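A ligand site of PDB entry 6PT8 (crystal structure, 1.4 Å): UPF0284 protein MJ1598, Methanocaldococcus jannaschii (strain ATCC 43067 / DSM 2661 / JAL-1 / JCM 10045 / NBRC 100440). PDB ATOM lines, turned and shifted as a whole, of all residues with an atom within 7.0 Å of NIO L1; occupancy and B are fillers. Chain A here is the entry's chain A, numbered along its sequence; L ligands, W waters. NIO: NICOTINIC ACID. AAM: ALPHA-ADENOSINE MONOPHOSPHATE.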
ATOM      1  N   PRO A  77      -6.534  17.764  -5.295  1.00  0.00           N
ATOM      2  CA  PRO A  77      -7.034  19.144  -5.276  1.00  0.00           C
ATOM      3  C   PRO A  77      -8.130  19.363  -4.251  1.00  0.00           C
ATOM      4  O   PRO A  77      -8.507  20.517  -4.028  1.00  0.00           O
ATOM      5  CB  PRO A  77      -7.525  19.350  -6.702  1.00  0.00           C
ATOM      6  CG  PRO A  77      -7.991  17.951  -7.125  1.00  0.00           C
ATOM      7  CD  PRO A  77      -7.044  16.981  -6.450  1.00  0.00           C
ATOM      8  N   GLU A 150     -16.741  18.092  -9.284  1.00  0.00           N
ATOM      9  CA  GLU A 150     -16.770  16.660  -9.533  1.00  0.00           C
ATOM     10  C   GLU A 150     -15.537  16.005  -8.939  1.00  0.00           C
ATOM     11  O   GLU A 150     -14.480  16.637  -8.770  1.00  0.00           O
ATOM     12  CB  GLU A 150     -16.789  16.325 -11.031  1.00  0.00           C
ATOM     13  CG  GLU A 150     -15.660  16.953 -11.860  1.00  0.00           C
ATOM     14  CD  GLU A 150     -14.253  16.362 -11.618  1.00  0.00           C
ATOM     15  OE1 GLU A 150     -13.274  17.152 -11.491  1.00  0.00           O
ATOM     16  OE2 GLU A 150     -14.121  15.114 -11.601  1.00  0.00           O
ATOM     17  N   VAL A 152     -14.210  12.426 -10.443  1.00  0.00           N
ATOM     18  CA  VAL A 152     -14.436  11.275 -11.296  1.00  0.00           C
ATOM     19  C   VAL A 152     -13.111  10.893 -11.951  1.00  0.00           C
ATOM     20  O   VAL A 152     -12.740  11.444 -13.006  1.00  0.00           O
ATOM     21  CB  VAL A 152     -15.491  11.559 -12.378  1.00  0.00           C
ATOM     22  CG1 VAL A 152     -15.748  10.285 -13.146  1.00  0.00           C
ATOM     23  CG2 VAL A 152     -16.794  12.102 -11.787  1.00  0.00           C
ATOM     24  N   GLY A 155     -12.451  10.870 -15.719  1.00  0.00           N
ATOM     25  CA  GLY A 155     -13.429  11.783 -16.278  1.00  0.00           C
ATOM     26  C   GLY A 155     -12.958  12.618 -17.456  1.00  0.00           C
ATOM     27  O   GLY A 155     -13.788  13.081 -18.227  1.00  0.00           O
ATOM     28  N   THR A 156     -11.657  12.817 -17.622  1.00  0.00           N
ATOM     29  CA  THR A 156     -11.233  13.505 -18.846  1.00  0.00           C
ATOM     30  C   THR A 156     -11.414  12.623 -20.075  1.00  0.00           C
ATOM     31  O   THR A 156     -11.588  13.159 -21.183  1.00  0.00           O
ATOM     32  CB  THR A 156      -9.814  14.084 -18.782  1.00  0.00           C
ATOM     33  OG1 THR A 156      -8.821  13.061 -18.622  1.00  0.00           O
ATOM     34  CG2 THR A 156      -9.679  15.110 -17.639  1.00  0.00           C
ATOM     35  N   ALA A 159     -15.186  12.784 -20.833  1.00  0.00           N
ATOM     36  CA  ALA A 159     -15.423  14.101 -21.417  1.00  0.00           C
ATOM     37  C   ALA A 159     -15.070  14.089 -22.904  1.00  0.00           C
ATOM     38  O   ALA A 159     -15.826  14.621 -23.734  1.00  0.00           O
ATOM     39  CB  ALA A 159     -14.609  15.157 -20.667  1.00  0.00           C
ATOM     40  N   LYS A 173      -7.705  17.893 -26.991  1.00  0.00           N
ATOM     41  CA  LYS A 173      -8.059  19.113 -26.260  1.00  0.00           C
ATOM     42  C   LYS A 173      -8.429  18.869 -24.797  1.00  0.00           C
ATOM     43  O   LYS A 173      -8.459  19.838 -24.020  1.00  0.00           O
ATOM     44  CB  LYS A 173      -9.211  19.848 -26.928  1.00  0.00           C
ATOM     45  CG  LYS A 173      -8.925  20.283 -28.345  1.00  0.00           C
ATOM     46  CD  LYS A 173      -9.946  21.292 -28.823  1.00  0.00           C
ATOM     47  CE  LYS A 173      -9.781  21.584 -30.298  1.00  0.00           C
ATOM     48  NZ  LYS A 173      -8.488  22.251 -30.574  1.00  0.00           N
ATOM     49  N   VAL A 174      -8.723  17.638 -24.402  1.00  0.00           N
ATOM     50  CA  VAL A 174      -9.053  17.390 -23.000  1.00  0.00           C
ATOM     51  C   VAL A 174      -7.767  17.358 -22.178  1.00  0.00           C
ATOM     52  O   VAL A 174      -6.686  17.059 -22.670  1.00  0.00           O
ATOM     53  CB  VAL A 174      -9.871  16.112 -22.763  1.00  0.00           C
ATOM     54  CG1 VAL A 174     -11.184  16.189 -23.463  1.00  0.00           C
ATOM     55  CG2 VAL A 174      -9.084  14.863 -23.173  1.00  0.00           C
ATOM     56  N   SER A 175      -7.911  17.660 -20.911  1.00  0.00           N
ATOM     57  CA  SER A 175      -6.765  17.758 -20.009  1.00  0.00           C
ATOM     58  C   SER A 175      -6.513  16.408 -19.360  1.00  0.00           C
ATOM     59  O   SER A 175      -6.893  15.352 -19.887  1.00  0.00           O
ATOM     60  CB  SER A 175      -6.988  18.925 -19.044  1.00  0.00           C
ATOM     61  OG  SER A 175      -5.868  19.146 -18.193  1.00  0.00           O
ATOM     62  N   SER A 176      -5.816  16.399 -18.232  1.00  0.00           N
ATOM     63  CA  SER A 176      -5.476  15.146 -17.575  1.00  0.00           C
ATOM     64  C   SER A 176      -5.142  15.466 -16.128  1.00  0.00           C
ATOM     65  O   SER A 176      -4.615  16.537 -15.816  1.00  0.00           O
ATOM     66  CB  SER A 176      -4.265  14.455 -18.223  1.00  0.00           C
ATOM     67  OG  SER A 176      -3.141  15.297 -18.180  1.00  0.00           O
ATOM     68  N   GLY A 177      -5.432  14.512 -15.264  1.00  0.00           N
ATOM     69  CA  GLY A 177      -5.168  14.705 -13.849  1.00  0.00           C
ATOM     70  C   GLY A 177      -3.744  14.507 -13.410  1.00  0.00           C
ATOM     71  O   GLY A 177      -3.473  14.489 -12.201  1.00  0.00           O
ATOM     72  N   SER A 178      -2.814  14.311 -14.352  1.00  0.00           N
ATOM     73  CA  SER A 178      -1.390  14.260 -14.025  1.00  0.00           C
ATOM     74  C   SER A 178      -0.612  14.763 -15.223  1.00  0.00           C
ATOM     75  O   SER A 178      -1.178  15.214 -16.217  1.00  0.00           O
ATOM     76  CB  SER A 178      -0.948  12.868 -13.592  1.00  0.00           C
ATOM     77  OG  SER A 178       0.325  12.912 -12.925  1.00  0.00           O
ATOM     78  N   GLY A 238     -14.896  22.857 -12.663  1.00  0.00           N
ATOM     79  CA  GLY A 238     -14.023  21.830 -13.194  1.00  0.00           C
ATOM     80  C   GLY A 238     -13.469  22.343 -14.493  1.00  0.00           C
ATOM     81  O   GLY A 238     -13.735  23.477 -14.913  1.00  0.00           O
ATOM     82  N   GLY A 239     -12.693  21.486 -15.146  1.00  0.00           N
ATOM     83  CA  GLY A 239     -11.965  21.901 -16.338  1.00  0.00           C
ATOM     84  C   GLY A 239     -12.602  21.388 -17.602  1.00  0.00           C
ATOM     85  O   GLY A 239     -13.774  21.667 -17.890  1.00  0.00           O
ATOM     86  N   THR A 240     -11.838  20.654 -18.404  1.00  0.00           N
ATOM     87  CA  THR A 240     -12.394  20.099 -19.627  1.00  0.00           C
ATOM     88  C   THR A 240     -13.558  19.136 -19.363  1.00  0.00           C
ATOM     89  O   THR A 240     -14.451  18.994 -20.196  1.00  0.00           O
ATOM     90  CB  THR A 240     -11.282  19.492 -20.498  1.00  0.00           C
ATOM     91  OG1 THR A 240     -10.622  18.432 -19.814  1.00  0.00           O
ATOM     92  CG2 THR A 240     -10.236  20.530 -20.828  1.00  0.00           C
ATOM     93  N   GLN A 241     -13.603  18.502 -18.189  1.00  0.00           N
ATOM     94  CA  GLN A 241     -14.778  17.722 -17.846  1.00  0.00           C
ATOM     95  C   GLN A 241     -16.050  18.577 -17.848  1.00  0.00           C
ATOM     96  O   GLN A 241     -17.113  18.141 -18.310  1.00  0.00           O
ATOM     97  CB  GLN A 241     -14.613  17.076 -16.472  1.00  0.00           C
ATOM     98  CG  GLN A 241     -13.543  15.985 -16.449  1.00  0.00           C
ATOM     99  CD  GLN A 241     -13.413  15.383 -15.091  1.00  0.00           C
ATOM    100  OE1 GLN A 241     -12.387  15.580 -14.426  1.00  0.00           O
ATOM    101  NE2 GLN A 241     -14.444  14.688 -14.652  1.00  0.00           N
ATOM    102  N   MET A 242     -15.981  19.793 -17.287  1.00  0.00           N
ATOM    103  CA  MET A 242     -17.145  20.671 -17.281  1.00  0.00           C
ATOM    104  C   MET A 242     -17.461  21.223 -18.655  1.00  0.00           C
ATOM    105  O   MET A 242     -18.605  21.636 -18.901  1.00  0.00           O
ATOM    106  CB  MET A 242     -16.946  21.772 -16.238  1.00  0.00           C
ATOM    107  CG  MET A 242     -17.033  21.248 -14.813  1.00  0.00           C
ATOM    108  SD  MET A 242     -18.605  20.422 -14.451  1.00  0.00           S
ATOM    109  CE  MET A 242     -18.263  19.789 -12.787  1.00  0.00           C
ATOM    110  N   SER A 243     -16.521  21.238 -19.606  1.00  0.00           N
ATOM    111  CA  SER A 243     -16.888  21.598 -20.966  1.00  0.00           C
ATOM    112  C   SER A 243     -17.784  20.539 -21.603  1.00  0.00           C
ATOM    113  O   SER A 243     -18.694  20.871 -22.374  1.00  0.00           O
ATOM    114  CB  SER A 243     -15.641  21.874 -21.812  1.00  0.00           C
ATOM    115  OG  SER A 243     -14.978  20.693 -22.242  1.00  0.00           O
ATOM    116  N   THR A 266     -12.452  27.124 -13.298  1.00  0.00           N
ATOM    117  CA  THR A 266     -11.345  26.173 -13.278  1.00  0.00           C
ATOM    118  C   THR A 266     -10.105  26.840 -12.708  1.00  0.00           C
ATOM    119  O   THR A 266     -10.184  27.910 -12.089  1.00  0.00           O
ATOM    120  CB  THR A 266     -11.146  25.573 -14.680  1.00  0.00           C
ATOM    121  OG1 THR A 266     -10.290  24.444 -14.613  1.00  0.00           O
ATOM    122  CG2 THR A 266     -10.553  26.575 -15.664  1.00  0.00           C
ATOM    123  N   VAL A 270      -5.386  24.324 -15.666  1.00  0.00           N
ATOM    124  CA  VAL A 270      -6.138  23.777 -16.791  1.00  0.00           C
ATOM    125  C   VAL A 270      -6.181  24.759 -17.949  1.00  0.00           C
ATOM    126  O   VAL A 270      -5.971  24.399 -19.115  1.00  0.00           O
ATOM    127  CB  VAL A 270      -7.553  23.350 -16.338  1.00  0.00           C
ATOM    128  CG1 VAL A 270      -8.416  22.945 -17.573  1.00  0.00           C
ATOM    129  CG2 VAL A 270      -7.477  22.220 -15.369  1.00  0.00           C
ATOM    130  N   ASP A 273      -2.877  24.759 -19.762  1.00  0.00           N
ATOM    131  CA  ASP A 273      -2.342  23.431 -20.045  1.00  0.00           C
ATOM    132  C   ASP A 273      -2.003  23.368 -21.521  1.00  0.00           C
ATOM    133  O   ASP A 273      -2.888  23.402 -22.376  1.00  0.00           O
ATOM    134  CB  ASP A 273      -3.407  22.386 -19.690  1.00  0.00           C
ATOM    135  CG  ASP A 273      -2.959  20.952 -19.946  1.00  0.00           C
ATOM    136  OD1 ASP A 273      -1.779  20.725 -20.282  1.00  0.00           O
ATOM    137  OD2 ASP A 273      -3.781  20.024 -19.791  1.00  0.00           O
ATOM    138  N   LEU A 278      -8.874  23.910 -23.409  1.00  0.00           N
ATOM    139  CA  LEU A 278     -10.183  24.194 -22.852  1.00  0.00           C
ATOM    140  C   LEU A 278     -10.888  25.299 -23.622  1.00  0.00           C
ATOM    141  O   LEU A 278     -12.061  25.172 -23.987  1.00  0.00           O
ATOM    142  CB  LEU A 278     -10.051  24.564 -21.375  1.00  0.00           C
ATOM    143  CG  LEU A 278     -11.349  24.972 -20.702  1.00  0.00           C
ATOM    144  CD1 LEU A 278     -12.380  23.859 -20.759  1.00  0.00           C
ATOM    145  CD2 LEU A 278     -11.064  25.381 -19.247  1.00  0.00           C
ATOM    146  N   GLY A 311       2.173  20.397 -14.144  1.00  0.00           N
ATOM    147  CA  GLY A 311       1.102  19.598 -14.713  1.00  0.00           C
ATOM    148  C   GLY A 311       0.553  18.524 -13.807  1.00  0.00           C
ATOM    149  O   GLY A 311      -0.389  17.829 -14.207  1.00  0.00           O
ATOM    150  N   VAL A 313      -1.831  16.997 -11.154  1.00  0.00           N
ATOM    151  CA  VAL A 313      -3.188  17.256 -10.627  1.00  0.00           C
ATOM    152  C   VAL A 313      -4.003  18.226 -11.457  1.00  0.00           C
ATOM    153  O   VAL A 313      -5.006  17.852 -12.070  1.00  0.00           O
ATOM    154  CB  VAL A 313      -3.173  17.679  -9.138  1.00  0.00           C
ATOM    155  CG1 VAL A 313      -4.601  17.929  -8.668  1.00  0.00           C
ATOM    156  CG2 VAL A 313      -2.486  16.636  -8.282  1.00  0.00           C
ATOM    157  N   LYS A 314      -3.634  19.514 -11.400  1.00  0.00           N
ATOM    158  CA  LYS A 314      -4.209  20.633 -12.117  1.00  0.00           C
ATOM    159  C   LYS A 314      -5.540  21.138 -11.554  1.00  0.00           C
ATOM    160  O   LYS A 314      -5.735  22.343 -11.410  1.00  0.00           O
ATOM    161  CB  LYS A 314      -4.430  20.368 -13.611  1.00  0.00           C
ATOM    162  CG  LYS A 314      -3.191  19.974 -14.386  1.00  0.00           C
ATOM    163  CD  LYS A 314      -3.520  19.894 -15.866  1.00  0.00           C
ATOM    164  CE  LYS A 314      -2.372  19.352 -16.700  1.00  0.00           C
ATOM    165  NZ  LYS A 314      -2.095  17.921 -16.396  1.00  0.00           N
ATOM    166  N   GLU A 315      -6.478  20.230 -11.276  1.00  0.00           N
ATOM    167  CA  GLU A 315      -7.870  20.573 -11.029  1.00  0.00           C
ATOM    168  C   GLU A 315      -8.560  19.364 -10.423  1.00  0.00           C
ATOM    169  O   GLU A 315      -8.058  18.237 -10.481  1.00  0.00           O
ATOM    170  CB  GLU A 315      -8.564  20.977 -12.337  1.00  0.00           C
ATOM    171  CG  GLU A 315     -10.085  21.170 -12.315  1.00  0.00           C
ATOM    172  CD  GLU A 315     -10.522  22.328 -11.485  1.00  0.00           C
ATOM    173  OE1 GLU A 315     -10.591  22.212 -10.249  1.00  0.00           O
ATOM    174  OE2 GLU A 315     -10.842  23.369 -12.103  1.00  0.00           O
ATOM    175  N   GLY A 316      -9.705  19.617  -9.798  1.00  0.00           N
ATOM    176  CA  GLY A 316     -10.606  18.565  -9.372  1.00  0.00           C
ATOM    177  C   GLY A 316     -11.272  18.911  -8.053  1.00  0.00           C
ATOM    178  O   GLY A 316     -10.851  19.805  -7.309  1.00  0.00           O
ATOM    179  N   VAL A 317     -12.339  18.182  -7.750  1.00  0.00           N
ATOM    180  CA  VAL A 317     -13.080  18.362  -6.517  1.00  0.00           C
ATOM    181  C   VAL A 317     -13.562  19.817  -6.412  1.00  0.00           C
ATOM    182  O   VAL A 317     -13.676  20.381  -5.321  1.00  0.00           O
ATOM    183  CB  VAL A 317     -12.282  17.926  -5.281  1.00  0.00           C
ATOM    184  CG1 VAL A 317     -13.226  17.703  -4.102  1.00  0.00           C
ATOM    185  CG2 VAL A 317     -11.514  16.633  -5.546  1.00  0.00           C
HETATM  186  N   NIO L   1      -9.170  17.070 -13.125  1.00  0.00           N
HETATM  187  C1  NIO L   1      -9.949  17.535 -14.120  1.00  0.00           C
HETATM  188  C2  NIO L   1      -9.386  18.114 -15.236  1.00  0.00           C
HETATM  189  C3  NIO L   1      -8.010  18.204 -15.369  1.00  0.00           C
HETATM  190  C4  NIO L   1      -7.237  17.736 -14.380  1.00  0.00           C
HETATM  191  C5  NIO L   1      -7.817  17.157 -13.260  1.00  0.00           C
HETATM  192  C6  NIO L   1     -10.290  18.633 -16.328  1.00  0.00           C
HETATM  193  O1  NIO L   1      -9.786  19.076 -17.384  1.00  0.00           O
HETATM  194  O2  NIO L   1     -11.541  18.595 -16.158  1.00  0.00           O
HETATM  195  C8A AAM L   2      -9.720  14.268  -8.197  1.00  0.00           C
HETATM  196  N9A AAM L   2      -9.165  13.807  -7.070  1.00  0.00           N
HETATM  197  C4A AAM L   2      -7.766  13.704  -7.388  1.00  0.00           C
HETATM  198  C5A AAM L   2      -7.574  14.138  -8.726  1.00  0.00           C
HETATM  199  N7A AAM L   2      -8.836  14.451  -9.171  1.00  0.00           N
HETATM  200  N3A AAM L   2      -6.792  13.276  -6.608  1.00  0.00           N
HETATM  201  C2A AAM L   2      -5.562  13.287  -7.113  1.00  0.00           C
HETATM  202  N1A AAM L   2      -5.274  13.664  -8.371  1.00  0.00           N
HETATM  203  C6A AAM L   2      -6.266  14.100  -9.182  1.00  0.00           C
HETATM  204  N6A AAM L   2      -5.946  14.470 -10.507  1.00  0.00           N
HETATM  205  P   AAM L   2      -8.219  11.970 -15.060  1.00  0.00           P
HETATM  206  O1P AAM L   2      -6.789  12.017 -15.511  1.00  0.00           O
HETATM  207  O2P AAM L   2      -9.137  11.916 -16.205  1.00  0.00           O
HETATM  208  O3P AAM L   2      -8.521  10.864 -14.134  1.00  0.00           O
HETATM  209  O6' AAM L   2      -8.414  13.382 -14.258  1.00  0.00           O
HETATM  210  C5' AAM L   2      -9.652  13.622 -13.599  1.00  0.00           C
HETATM  211  C4' AAM L   2      -9.565  13.347 -12.135  1.00  0.00           C
HETATM  212  O5' AAM L   2      -8.560  14.253 -11.529  1.00  0.00           O
HETATM  213  C3' AAM L   2     -10.852  13.668 -11.395  1.00  0.00           C
HETATM  214  O3' AAM L   2     -10.963  12.744 -10.334  1.00  0.00           O
HETATM  215  C2' AAM L   2     -10.633  15.039 -10.913  1.00  0.00           C
HETATM  216  O2' AAM L   2     -11.517  15.440  -9.873  1.00  0.00           O
HETATM  217  C1' AAM L   2      -9.192  15.011 -10.454  1.00  0.00           C
HETATM  218  O   HOH W   1     -13.114  18.880 -13.741  1.00  0.00           O
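Water W1 lies within hydrogen-bond range of the side-chain carboxylate of Glu 150 (2.8 Å), an oxygen (O2) of NIO L1 (2.9 Å), the backbone NH of Gly 239 (3.0 Å) and the side-chain amide oxygen of Gln 241 (3.4 Å).
The side-chain hydroxyl (OG1) of Thr 240 lies within hydrogen-bond range of the backbone NH (N) of Ser 175 (3.0 Å). The backbone carbonyl oxygen (O) of Ser 176 lies within hydrogen-bond range of the side-chain amino group (NZ) of Lys 314, at 2.9 Å. The backbone carbonyl oxygen (O) of Gly 177 lies within hydrogen-bond range of the backbone NH (N) of Val 313 (3.2 Å). The side-chain amide nitrogen (NE2) of Gln 241 sits at hydrogen-bond distance from the side-chain carboxylate (OE2) of Glu 150 (3.1 Å). OG of Ser 176 lies within hydrogen-bond range of O of Ser 178 (2.8 Å). NZ of Lys 314 sits at hydrogen-bond distance from O of Ser 178. O of Thr 240 lies within hydrogen-bond range of OG of Ser 243. O of Ser 175 is in hydrogen-bond range of OG1 of Thr 156 (3.3 Å).
N of NIO L1 lies close to O of Glu 315 (3.1 Å). Merely in contact with NIO L1: Val 313 (3.1 Å), Ser 176 (3.2 Å), Ser 175 (3.3 Å), Gly 177 (3.7 Å), Thr 156 (3.8 Å) and Lys 314 (3.9 Å). Of the 28 residues printed, 10 come within 4 Å of NIO L1. The nearest printed residue that does not touch NIO L1 is Val 270 (4.1 Å).
The backbone carbonyl oxygen (O) of Gly 177 is in hydrogen-bond range of a nitrogen (N6A) of AAM L2. O1P of AAM L2 sits at hydrogen-bond distance from N of Gly 177 (2.9 Å). O2P of AAM L2 is in hydrogen-bond range of N of Thr 156 (3.0 Å). The side-chain carboxylate of Glu 150 sits at hydrogen-bond distance from an oxygen (O2') of AAM L2 (2.9 Å). The backbone NH (N) of Thr 240 is in hydrogen-bond range of an oxygen (O1) of NIO L1 (2.8 Å). The backbone NH (N) of Val 152 lies close to an oxygen (O3') of AAM L2 (3.3 Å). N of Gln 241 sits at hydrogen-bond distance from O2 of NIO L1 (2.9 Å). An oxygen (O2') of AAM L2 lies close to the backbone carbonyl oxygen of Glu 150 (3.4 Å). O1 of NIO L1 lies within hydrogen-bond range of OG1 of Thr 240 (2.6 Å). O3' of AAM L2 sits close to O of Val 152 (3.5 Å). OG1 of Thr 156 lies within hydrogen-bond range of O2P of AAM L2, 2.7 Å away. An oxygen (O2) of NIO L1 sits at hydrogen-bond distance from the backbone NH of Gly 239, at 3.3 Å.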
